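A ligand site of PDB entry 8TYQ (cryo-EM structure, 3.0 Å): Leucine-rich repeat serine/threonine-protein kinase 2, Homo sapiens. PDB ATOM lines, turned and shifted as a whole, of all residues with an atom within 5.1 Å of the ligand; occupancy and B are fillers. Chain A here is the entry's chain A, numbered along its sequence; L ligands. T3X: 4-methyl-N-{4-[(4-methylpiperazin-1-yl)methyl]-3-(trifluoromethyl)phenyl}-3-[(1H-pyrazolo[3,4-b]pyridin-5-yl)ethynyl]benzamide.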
ATOM      1  N   LEU A1885       0.748  24.105  13.265  1.00  0.00           N
ATOM      2  CA  LEU A1885       0.286  23.660  14.564  1.00  0.00           C
ATOM      3  C   LEU A1885      -0.193  22.213  14.487  1.00  0.00           C
ATOM      4  O   LEU A1885      -0.906  21.830  13.555  1.00  0.00           O
ATOM      5  CB  LEU A1885      -0.824  24.583  15.061  1.00  0.00           C
ATOM      6  CG  LEU A1885      -1.383  24.286  16.454  1.00  0.00           C
ATOM      7  CD1 LEU A1885      -0.457  24.875  17.493  1.00  0.00           C
ATOM      8  CD2 LEU A1885      -2.748  24.900  16.584  1.00  0.00           C
ATOM      9  N   PHE A1890      -4.474  19.381  12.760  1.00  0.00           N
ATOM     10  CA  PHE A1890      -5.666  20.189  13.016  1.00  0.00           C
ATOM     11  C   PHE A1890      -6.158  20.892  11.761  1.00  0.00           C
ATOM     12  O   PHE A1890      -6.880  21.892  11.872  1.00  0.00           O
ATOM     13  CB  PHE A1890      -5.368  21.194  14.118  1.00  0.00           C
ATOM     14  CG  PHE A1890      -4.892  20.571  15.400  1.00  0.00           C
ATOM     15  CD1 PHE A1890      -5.699  19.694  16.090  1.00  0.00           C
ATOM     16  CD2 PHE A1890      -3.611  20.809  15.863  1.00  0.00           C
ATOM     17  CE1 PHE A1890      -5.260  19.109  17.253  1.00  0.00           C
ATOM     18  CE2 PHE A1890      -3.167  20.216  17.021  1.00  0.00           C
ATOM     19  CZ  PHE A1890      -3.992  19.366  17.717  1.00  0.00           C
ATOM     20  N   VAL A1893      -3.746  24.939  10.229  1.00  0.00           N
ATOM     21  CA  VAL A1893      -3.673  25.813  11.396  1.00  0.00           C
ATOM     22  C   VAL A1893      -2.204  26.017  11.743  1.00  0.00           C
ATOM     23  O   VAL A1893      -1.439  25.045  11.802  1.00  0.00           O
ATOM     24  CB  VAL A1893      -4.456  25.253  12.592  1.00  0.00           C
ATOM     25  CG1 VAL A1893      -4.406  26.218  13.761  1.00  0.00           C
ATOM     26  CG2 VAL A1893      -5.902  24.995  12.204  1.00  0.00           C
ATOM     27  N   ALA A1904      -3.649  30.843  17.624  1.00  0.00           N
ATOM     28  CA  ALA A1904      -3.732  29.875  16.532  1.00  0.00           C
ATOM     29  C   ALA A1904      -4.469  30.497  15.348  1.00  0.00           C
ATOM     30  O   ALA A1904      -5.466  31.188  15.540  1.00  0.00           O
ATOM     31  CB  ALA A1904      -4.452  28.604  16.977  1.00  0.00           C
ATOM     32  N   VAL A1905      -3.970  30.264  14.136  1.00  0.00           N
ATOM     33  CA  VAL A1905      -4.544  30.854  12.935  1.00  0.00           C
ATOM     34  C   VAL A1905      -4.850  29.755  11.930  1.00  0.00           C
ATOM     35  O   VAL A1905      -3.944  29.089  11.437  1.00  0.00           O
ATOM     36  CB  VAL A1905      -3.603  31.895  12.312  1.00  0.00           C
ATOM     37  CG1 VAL A1905      -4.052  32.236  10.908  1.00  0.00           C
ATOM     38  CG2 VAL A1905      -3.555  33.151  13.169  1.00  0.00           C
ATOM     39  N   LYS A1906      -6.132  29.575  11.630  1.00  0.00           N
ATOM     40  CA  LYS A1906      -6.575  28.683  10.563  1.00  0.00           C
ATOM     41  C   LYS A1906      -6.820  29.520   9.307  1.00  0.00           C
ATOM     42  O   LYS A1906      -7.683  30.405   9.306  1.00  0.00           O
ATOM     43  CB  LYS A1906      -7.852  27.937  10.951  1.00  0.00           C
ATOM     44  CG  LYS A1906      -8.497  27.208   9.780  1.00  0.00           C
ATOM     45  CD  LYS A1906      -9.864  26.655  10.132  1.00  0.00           C
ATOM     46  CE  LYS A1906     -10.097  25.300   9.502  1.00  0.00           C
ATOM     47  NZ  LYS A1906     -11.372  24.698   9.941  1.00  0.00           N
ATOM     48  N   GLU A1920     -19.303  28.534   9.435  1.00  0.00           N
ATOM     49  CA  GLU A1920     -18.585  28.272  10.670  1.00  0.00           C
ATOM     50  C   GLU A1920     -18.662  29.465  11.603  1.00  0.00           C
ATOM     51  O   GLU A1920     -18.779  29.295  12.820  1.00  0.00           O
ATOM     52  CB  GLU A1920     -17.136  27.911  10.354  1.00  0.00           C
ATOM     53  CG  GLU A1920     -16.365  27.311  11.515  1.00  0.00           C
ATOM     54  CD  GLU A1920     -15.172  26.516  11.050  1.00  0.00           C
ATOM     55  OE1 GLU A1920     -14.995  26.357   9.818  1.00  0.00           O
ATOM     56  OE2 GLU A1920     -14.406  26.029  11.900  1.00  0.00           O
ATOM     57  N   VAL A1923     -22.082  29.497  13.262  1.00  0.00           N
ATOM     58  CA  VAL A1923     -22.149  28.515  14.343  1.00  0.00           C
ATOM     59  C   VAL A1923     -21.363  28.992  15.566  1.00  0.00           C
ATOM     60  O   VAL A1923     -21.833  28.904  16.697  1.00  0.00           O
ATOM     61  CB  VAL A1923     -21.662  27.138  13.864  1.00  0.00           C
ATOM     62  CG1 VAL A1923     -21.750  26.151  14.995  1.00  0.00           C
ATOM     63  CG2 VAL A1923     -22.498  26.665  12.691  1.00  0.00           C
ATOM     64  N   LEU A1924     -20.163  29.528  15.346  1.00  0.00           N
ATOM     65  CA  LEU A1924     -19.278  29.869  16.458  1.00  0.00           C
ATOM     66  C   LEU A1924     -19.780  31.073  17.238  1.00  0.00           C
ATOM     67  O   LEU A1924     -19.601  31.144  18.462  1.00  0.00           O
ATOM     68  CB  LEU A1924     -17.860  30.123  15.947  1.00  0.00           C
ATOM     69  CG  LEU A1924     -17.031  28.900  15.616  1.00  0.00           C
ATOM     70  CD1 LEU A1924     -15.750  29.306  14.918  1.00  0.00           C
ATOM     71  CD2 LEU A1924     -16.732  28.183  16.909  1.00  0.00           C
ATOM     72  N   LEU A1927     -21.975  30.196  20.353  1.00  0.00           N
ATOM     73  CA  LEU A1927     -21.516  29.155  21.276  1.00  0.00           C
ATOM     74  C   LEU A1927     -20.501  29.772  22.232  1.00  0.00           C
ATOM     75  O   LEU A1927     -19.347  30.010  21.861  1.00  0.00           O
ATOM     76  CB  LEU A1927     -20.904  27.985  20.511  1.00  0.00           C
ATOM     77  CG  LEU A1927     -21.858  27.312  19.534  1.00  0.00           C
ATOM     78  CD1 LEU A1927     -21.141  26.254  18.720  1.00  0.00           C
ATOM     79  CD2 LEU A1927     -23.033  26.707  20.272  1.00  0.00           C
ATOM     80  N   LEU A1932     -16.124  24.937  25.125  1.00  0.00           N
ATOM     81  CA  LEU A1932     -16.171  25.193  23.690  1.00  0.00           C
ATOM     82  C   LEU A1932     -15.049  26.158  23.331  1.00  0.00           C
ATOM     83  O   LEU A1932     -14.882  27.193  23.975  1.00  0.00           O
ATOM     84  CB  LEU A1932     -17.517  25.770  23.278  1.00  0.00           C
ATOM     85  CG  LEU A1932     -18.737  24.898  23.582  1.00  0.00           C
ATOM     86  CD1 LEU A1932     -20.024  25.682  23.414  1.00  0.00           C
ATOM     87  CD2 LEU A1932     -18.746  23.691  22.668  1.00  0.00           C
ATOM     88  N   ILE A1933     -14.283  25.811  22.295  1.00  0.00           N
ATOM     89  CA  ILE A1933     -13.137  26.631  21.911  1.00  0.00           C
ATOM     90  C   ILE A1933     -13.610  28.031  21.558  1.00  0.00           C
ATOM     91  O   ILE A1933     -14.568  28.209  20.787  1.00  0.00           O
ATOM     92  CB  ILE A1933     -12.362  25.957  20.762  1.00  0.00           C
ATOM     93  CG1 ILE A1933     -11.087  26.743  20.437  1.00  0.00           C
ATOM     94  CG2 ILE A1933     -13.239  25.785  19.541  1.00  0.00           C
ATOM     95  CD1 ILE A1933     -10.008  26.620  21.479  1.00  0.00           C
ATOM     96  N   LEU A1945      -9.272  32.460  10.614  1.00  0.00           N
ATOM     97  CA  LEU A1945      -9.848  32.373  11.956  1.00  0.00           C
ATOM     98  C   LEU A1945      -8.719  32.320  12.981  1.00  0.00           C
ATOM     99  O   LEU A1945      -7.693  31.676  12.745  1.00  0.00           O
ATOM    100  CB  LEU A1945     -10.745  31.150  12.101  1.00  0.00           C
ATOM    101  CG  LEU A1945     -12.127  31.266  11.485  1.00  0.00           C
ATOM    102  CD1 LEU A1945     -12.831  29.928  11.455  1.00  0.00           C
ATOM    103  CD2 LEU A1945     -12.886  32.242  12.343  1.00  0.00           C
ATOM    104  N   MET A1947      -7.668  31.640  17.159  1.00  0.00           N
ATOM    105  CA  MET A1947      -8.300  31.198  18.430  1.00  0.00           C
ATOM    106  C   MET A1947      -7.268  30.799  19.478  1.00  0.00           C
ATOM    107  O   MET A1947      -6.221  30.431  19.018  1.00  0.00           O
ATOM    108  CB  MET A1947      -9.121  29.980  18.068  1.00  0.00           C
ATOM    109  CG  MET A1947     -10.254  30.241  17.137  1.00  0.00           C
ATOM    110  SD  MET A1947     -11.779  29.567  17.732  1.00  0.00           S
ATOM    111  CE  MET A1947     -12.758  29.768  16.264  1.00  0.00           C
ATOM    112  N   GLU A1948      -7.585  30.753  20.785  1.00  0.00           N
ATOM    113  CA  GLU A1948      -6.674  30.395  21.898  1.00  0.00           C
ATOM    114  C   GLU A1948      -5.711  29.242  21.614  1.00  0.00           C
ATOM    115  O   GLU A1948      -6.182  28.273  21.089  1.00  0.00           O
ATOM    116  CB  GLU A1948      -7.515  29.832  22.996  1.00  0.00           C
ATOM    117  CG  GLU A1948      -8.723  30.628  23.296  1.00  0.00           C
ATOM    118  CD  GLU A1948      -9.412  29.923  24.434  1.00  0.00           C
ATOM    119  OE1 GLU A1948      -9.158  28.728  24.580  1.00  0.00           O
ATOM    120  OE2 GLU A1948     -10.181  30.564  25.171  1.00  0.00           O
ATOM    121  N   LEU A1949      -4.420  29.335  21.998  1.00  0.00           N
ATOM    122  CA  LEU A1949      -3.420  28.290  21.752  1.00  0.00           C
ATOM    123  C   LEU A1949      -3.509  27.324  22.870  1.00  0.00           C
ATOM    124  O   LEU A1949      -3.185  27.685  23.974  1.00  0.00           O
ATOM    125  CB  LEU A1949      -2.006  28.814  21.792  1.00  0.00           C
ATOM    126  CG  LEU A1949      -0.971  28.092  20.941  1.00  0.00           C
ATOM    127  CD1 LEU A1949      -1.523  26.861  20.279  1.00  0.00           C
ATOM    128  CD2 LEU A1949      -0.495  29.052  19.888  1.00  0.00           C
ATOM    129  N   ALA A1950      -4.103  26.198  22.594  1.00  0.00           N
ATOM    130  CA  ALA A1950      -3.935  25.184  23.626  1.00  0.00           C
ATOM    131  C   ALA A1950      -2.445  24.895  23.772  1.00  0.00           C
ATOM    132  O   ALA A1950      -1.822  24.312  22.878  1.00  0.00           O
ATOM    133  CB  ALA A1950      -4.720  23.930  23.294  1.00  0.00           C
ATOM    134  N   SER A1951      -1.869  25.291  24.908  1.00  0.00           N
ATOM    135  CA  SER A1951      -0.432  25.120  25.110  1.00  0.00           C
ATOM    136  C   SER A1951      -0.021  23.666  25.231  1.00  0.00           C
ATOM    137  O   SER A1951       1.127  23.328  24.912  1.00  0.00           O
ATOM    138  CB  SER A1951       0.011  25.886  26.358  1.00  0.00           C
ATOM    139  OG  SER A1951      -0.386  27.246  26.294  1.00  0.00           O
ATOM    140  N   GLY A1953      -1.300  20.953  23.632  1.00  0.00           N
ATOM    141  CA  GLY A1953      -1.763  20.111  22.549  1.00  0.00           C
ATOM    142  C   GLY A1953      -3.208  19.694  22.735  1.00  0.00           C
ATOM    143  O   GLY A1953      -3.989  20.334  23.440  1.00  0.00           O
ATOM    144  N   SER A1954      -3.562  18.597  22.084  1.00  0.00           N
ATOM    145  CA  SER A1954      -4.888  18.034  22.217  1.00  0.00           C
ATOM    146  C   SER A1954      -4.888  16.910  23.250  1.00  0.00           C
ATOM    147  O   SER A1954      -3.858  16.545  23.815  1.00  0.00           O
ATOM    148  CB  SER A1954      -5.397  17.533  20.867  1.00  0.00           C
ATOM    149  OG  SER A1954      -4.646  16.428  20.419  1.00  0.00           O
ATOM    150  N   LEU A1985     -24.109  21.733  23.763  1.00  0.00           N
ATOM    151  CA  LEU A1985     -24.443  21.641  22.350  1.00  0.00           C
ATOM    152  C   LEU A1985     -25.815  21.016  22.151  1.00  0.00           C
ATOM    153  O   LEU A1985     -26.594  21.467  21.301  1.00  0.00           O
ATOM    154  CB  LEU A1985     -23.385  20.831  21.601  1.00  0.00           C
ATOM    155  CG  LEU A1985     -22.064  21.528  21.291  1.00  0.00           C
ATOM    156  CD1 LEU A1985     -21.063  20.535  20.751  1.00  0.00           C
ATOM    157  CD2 LEU A1985     -22.287  22.665  20.308  1.00  0.00           C
ATOM    158  N   ILE A1990     -27.620  21.285  18.705  1.00  0.00           N
ATOM    159  CA  ILE A1990     -26.503  21.062  17.790  1.00  0.00           C
ATOM    160  C   ILE A1990     -26.001  19.652  18.017  1.00  0.00           C
ATOM    161  O   ILE A1990     -25.846  19.208  19.156  1.00  0.00           O
ATOM    162  CB  ILE A1990     -25.383  22.094  18.005  1.00  0.00           C
ATOM    163  CG1 ILE A1990     -25.880  23.494  17.648  1.00  0.00           C
ATOM    164  CG2 ILE A1990     -24.171  21.743  17.175  1.00  0.00           C
ATOM    165  CD1 ILE A1990     -24.943  24.588  18.068  1.00  0.00           C
ATOM    166  N   TYR A1992     -23.096  17.903  16.716  1.00  0.00           N
ATOM    167  CA  TYR A1992     -21.678  17.562  16.871  1.00  0.00           C
ATOM    168  C   TYR A1992     -21.465  16.093  16.512  1.00  0.00           C
ATOM    169  O   TYR A1992     -21.221  15.271  17.402  1.00  0.00           O
ATOM    170  CB  TYR A1992     -21.155  17.857  18.284  1.00  0.00           C
ATOM    171  CG  TYR A1992     -19.651  17.894  18.332  1.00  0.00           C
ATOM    172  CD1 TYR A1992     -18.956  19.040  17.997  1.00  0.00           C
ATOM    173  CD2 TYR A1992     -18.915  16.768  18.671  1.00  0.00           C
ATOM    174  CE1 TYR A1992     -17.595  19.076  18.030  1.00  0.00           C
ATOM    175  CE2 TYR A1992     -17.549  16.796  18.699  1.00  0.00           C
ATOM    176  CZ  TYR A1992     -16.888  17.957  18.370  1.00  0.00           C
ATOM    177  OH  TYR A1992     -15.527  17.993  18.402  1.00  0.00           O
ATOM    178  N   ARG A1993     -21.598  15.766  15.230  1.00  0.00           N
ATOM    179  CA  ARG A1993     -21.687  14.376  14.802  1.00  0.00           C
ATOM    180  C   ARG A1993     -20.565  13.504  15.366  1.00  0.00           C
ATOM    181  O   ARG A1993     -20.840  12.449  15.944  1.00  0.00           O
ATOM    182  CB  ARG A1993     -21.657  14.311  13.270  1.00  0.00           C
ATOM    183  CG  ARG A1993     -23.012  14.093  12.635  1.00  0.00           C
ATOM    184  CD  ARG A1993     -23.066  14.744  11.251  1.00  0.00           C
ATOM    185  NE  ARG A1993     -24.432  15.078  10.862  1.00  0.00           N
ATOM    186  CZ  ARG A1993     -25.178  16.011  11.437  1.00  0.00           C
ATOM    187  NH1 ARG A1993     -24.707  16.748  12.438  1.00  0.00           N
ATOM    188  NH2 ARG A1993     -26.416  16.221  11.012  1.00  0.00           N
ATOM    189  N   LEU A2001      -9.136  19.735  23.417  1.00  0.00           N
ATOM    190  CA  LEU A2001      -7.993  20.619  23.526  1.00  0.00           C
ATOM    191  C   LEU A2001      -7.676  20.885  24.987  1.00  0.00           C
ATOM    192  O   LEU A2001      -8.574  21.212  25.770  1.00  0.00           O
ATOM    193  CB  LEU A2001      -8.269  21.933  22.806  1.00  0.00           C
ATOM    194  CG  LEU A2001      -8.519  21.803  21.305  1.00  0.00           C
ATOM    195  CD1 LEU A2001      -8.678  23.174  20.700  1.00  0.00           C
ATOM    196  CD2 LEU A2001      -7.356  21.089  20.681  1.00  0.00           C
ATOM    197  N   ILE A2015     -13.715  21.455  23.649  1.00  0.00           N
ATOM    198  CA  ILE A2015     -14.018  20.641  22.474  1.00  0.00           C
ATOM    199  C   ILE A2015     -13.992  21.520  21.235  1.00  0.00           C
ATOM    200  O   ILE A2015     -14.397  22.692  21.271  1.00  0.00           O
ATOM    201  CB  ILE A2015     -15.375  19.923  22.649  1.00  0.00           C
ATOM    202  CG1 ILE A2015     -16.556  20.835  22.302  1.00  0.00           C
ATOM    203  CG2 ILE A2015     -15.527  19.405  24.062  1.00  0.00           C
ATOM    204  CD1 ILE A2015     -17.890  20.194  22.572  1.00  0.00           C
ATOM    205  N   ALA A2016     -13.483  20.981  20.134  1.00  0.00           N
ATOM    206  CA  ALA A2016     -13.271  21.720  18.903  1.00  0.00           C
ATOM    207  C   ALA A2016     -13.694  20.887  17.699  1.00  0.00           C
ATOM    208  O   ALA A2016     -13.976  19.692  17.810  1.00  0.00           O
ATOM    209  CB  ALA A2016     -11.799  22.133  18.752  1.00  0.00           C
ATOM    210  N   ASP A2017     -13.748  21.542  16.543  1.00  0.00           N
ATOM    211  CA  ASP A2017     -14.089  20.876  15.286  1.00  0.00           C
ATOM    212  C   ASP A2017     -13.282  21.529  14.181  1.00  0.00           C
ATOM    213  O   ASP A2017     -13.625  22.636  13.740  1.00  0.00           O
ATOM    214  CB  ASP A2017     -15.583  20.968  14.998  1.00  0.00           C
ATOM    215  CG  ASP A2017     -16.027  20.022  13.909  1.00  0.00           C
ATOM    216  OD1 ASP A2017     -15.156  19.500  13.172  1.00  0.00           O
ATOM    217  OD2 ASP A2017     -17.240  19.813  13.768  1.00  0.00           O
ATOM    218  N   TYR A2018     -12.236  20.851  13.720  1.00  0.00           N
ATOM    219  CA  TYR A2018     -11.329  21.406  12.723  1.00  0.00           C
ATOM    220  C   TYR A2018     -11.846  21.228  11.303  1.00  0.00           C
ATOM    221  O   TYR A2018     -11.243  21.775  10.370  1.00  0.00           O
ATOM    222  CB  TYR A2018      -9.963  20.738  12.852  1.00  0.00           C
ATOM    223  CG  TYR A2018      -9.592  20.463  14.285  1.00  0.00           C
ATOM    224  CD1 TYR A2018      -9.281  21.500  15.159  1.00  0.00           C
ATOM    225  CD2 TYR A2018      -9.568  19.168  14.782  1.00  0.00           C
ATOM    226  CE1 TYR A2018      -8.957  21.257  16.473  1.00  0.00           C
ATOM    227  CE2 TYR A2018      -9.239  18.917  16.092  1.00  0.00           C
ATOM    228  CZ  TYR A2018      -8.942  19.957  16.926  1.00  0.00           C
ATOM    229  OH  TYR A2018      -8.616  19.693  18.231  1.00  0.00           O
HETATM  230  C13 T3X L   1     -17.105  23.867  17.302  1.00  0.00           C
HETATM  231  C15 T3X L   1     -18.031  24.621  15.225  1.00  0.00           C
HETATM  232  C17 T3X L   1     -19.596  23.289  16.844  1.00  0.00           C
HETATM  233  C20 T3X L   1     -21.621  21.149  14.813  1.00  0.00           C
HETATM  234  C11 T3X L   1     -15.725  25.119  15.749  1.00  0.00           C
HETATM  235  C12 T3X L   1     -15.898  24.465  16.949  1.00  0.00           C
HETATM  236  C14 T3X L   1     -18.212  23.924  16.421  1.00  0.00           C
HETATM  237  C16 T3X L   1     -16.794  25.190  14.885  1.00  0.00           C
HETATM  238  C19 T3X L   1     -21.078  22.377  15.556  1.00  0.00           C
HETATM  239  N10 T3X L   1     -14.408  25.730  15.425  1.00  0.00           N
HETATM  240  C01 T3X L   1      -7.880  27.279  14.824  1.00  0.00           C
HETATM  241  C02 T3X L   1      -9.276  26.752  15.084  1.00  0.00           C
HETATM  242  C03 T3X L   1      -9.495  25.855  16.089  1.00  0.00           C
HETATM  243  C04 T3X L   1     -10.732  25.357  16.359  1.00  0.00           C
HETATM  244  C05 T3X L   1     -11.789  25.779  15.590  1.00  0.00           C
HETATM  245  C06 T3X L   1     -11.596  26.661  14.563  1.00  0.00           C
HETATM  246  C07 T3X L   1     -10.333  27.154  14.305  1.00  0.00           C
HETATM  247  C08 T3X L   1     -13.141  25.184  15.920  1.00  0.00           C
HETATM  248  C22 T3X L   1     -19.793  20.250  15.054  1.00  0.00           C
HETATM  249  C23 T3X L   1     -19.154  21.493  15.616  1.00  0.00           C
HETATM  250  C24 T3X L   1     -21.066  19.491  13.567  1.00  0.00           C
HETATM  251  C25 T3X L   1     -17.165  23.170  18.643  1.00  0.00           C
HETATM  252  C29 T3X L   1      -8.317  25.412  16.927  1.00  0.00           C
HETATM  253  C30 T3X L   1      -7.391  25.079  17.570  1.00  0.00           C
HETATM  254  C31 T3X L   1      -6.195  24.664  18.404  1.00  0.00           C
HETATM  255  C32 T3X L   1      -5.445  23.564  18.117  1.00  0.00           C
HETATM  256  C33 T3X L   1      -4.432  23.320  18.921  1.00  0.00           C
HETATM  257  C34 T3X L   1      -4.128  24.132  20.016  1.00  0.00           C
HETATM  258  C37 T3X L   1      -3.386  22.357  19.082  1.00  0.00           C
HETATM  259  C39 T3X L   1      -5.885  25.485  19.512  1.00  0.00           C
HETATM  260  F26 T3X L   1     -17.226  21.833  18.480  1.00  0.00           F
HETATM  261  F27 T3X L   1     -16.058  23.459  19.338  1.00  0.00           F
HETATM  262  F28 T3X L   1     -18.233  23.646  19.316  1.00  0.00           F
HETATM  263  N18 T3X L   1     -20.023  22.141  16.283  1.00  0.00           N
HETATM  264  N21 T3X L   1     -20.656  20.574  14.149  1.00  0.00           N
HETATM  265  N35 T3X L   1      -2.995  23.462  20.529  1.00  0.00           N
HETATM  266  N36 T3X L   1      -2.517  22.390  19.983  1.00  0.00           N
HETATM  267  N38 T3X L   1      -4.831  25.198  20.319  1.00  0.00           N
HETATM  268  O09 T3X L   1     -13.094  24.240  16.588  1.00  0.00           O
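F27 of the ligand sits close to O of Ile 2015, at 2.7 Å.
Leu 1885 touches the ligand.
Phe 1890 touches the ligand.
CG1 of Val 1893 touches C01 of the ligand, 3.8 Å away.
CB of Lys 1906 touches C01 of the ligand, 3.9 Å away.
Glu 1920 touches the ligand (OE2 to N10, 3.5 Å).
Val 1923 touches the ligand.
Leu 1924 touches the ligand.
Leu 1927 touches the ligand.
Leu 1932 touches the ligand.
Ile 1933 touches the ligand (CG2 to O09, 3.3 Å).
Met 1947 touches the ligand.
C of Leu 1949 touches N38 of the ligand, at 3.6 Å.
Gly 1953 touches the ligand.
Ile 1990 touches the ligand.
Tyr 1992 touches the ligand (CE1 to F26, 2.8 Å).
CD1 of Leu 2001 touches C31 of the ligand, at 3.7 Å.
Ala 2016 touches the ligand (CB to O09, 3.3 Å).
Hydrophobic or aromatic side chains within 4 Å of the ligand: Leu 1885, Phe 1890, Val 1893, Val 1923, Leu 1924, Leu 1927, Leu 1932, Ile 1933, Met 1947, Leu 1949, Ala 1950, Ile 1990, Tyr 1992, Leu 2001, Ile 2015 and Ala 2016.
Of the 29 residues printed, 21 come within 4 Å of the ligand.
N21 of the ligand lies within salt-bridge range of OD2 of Asp 2017, at 3.5 Å.
O of Glu 1948 sits close to N38 of the ligand (3.4 Å).
The backbone carbonyl oxygen (O) of Ala 1950 sits at hydrogen-bond distance from a nitrogen (N35) of the ligand, 2.8 Å away.
N of Ala 1950 lies within hydrogen-bond range of N38 of the ligand (2.6 Å).
The backbone NH of Asp 2017 sits at hydrogen-bond distance from an oxygen (O09) of the ligand.
NZ of Lys 1906 is in hydrogen-bond range of O of Tyr 2018, 3.0 Å away.
The backbone NH (N) of Lys 1906 lies within hydrogen-bond range of the backbone carbonyl oxygen (O) of Leu 1945 (2.8 Å).
The backbone NH (N) of Met 1947 is in hydrogen-bond range of the backbone carbonyl oxygen (O) of Ala 1904 (2.8 Å).
The backbone carbonyl oxygen (O) of Ile 2015 sits at hydrogen-bond distance from the backbone NH (N) of Ile 1933 (3.3 Å).
O of Val 1893 is in hydrogen-bond range of N of Leu 1885 (2.8 Å).
OE2 of Glu 1920 lies within salt-bridge range of NZ of Lys 1906, at 3.8 Å.
The backbone NH (N) of Ile 1990 is in hydrogen-bond range of the backbone carbonyl oxygen (O) of Leu 1985 (2.8 Å).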
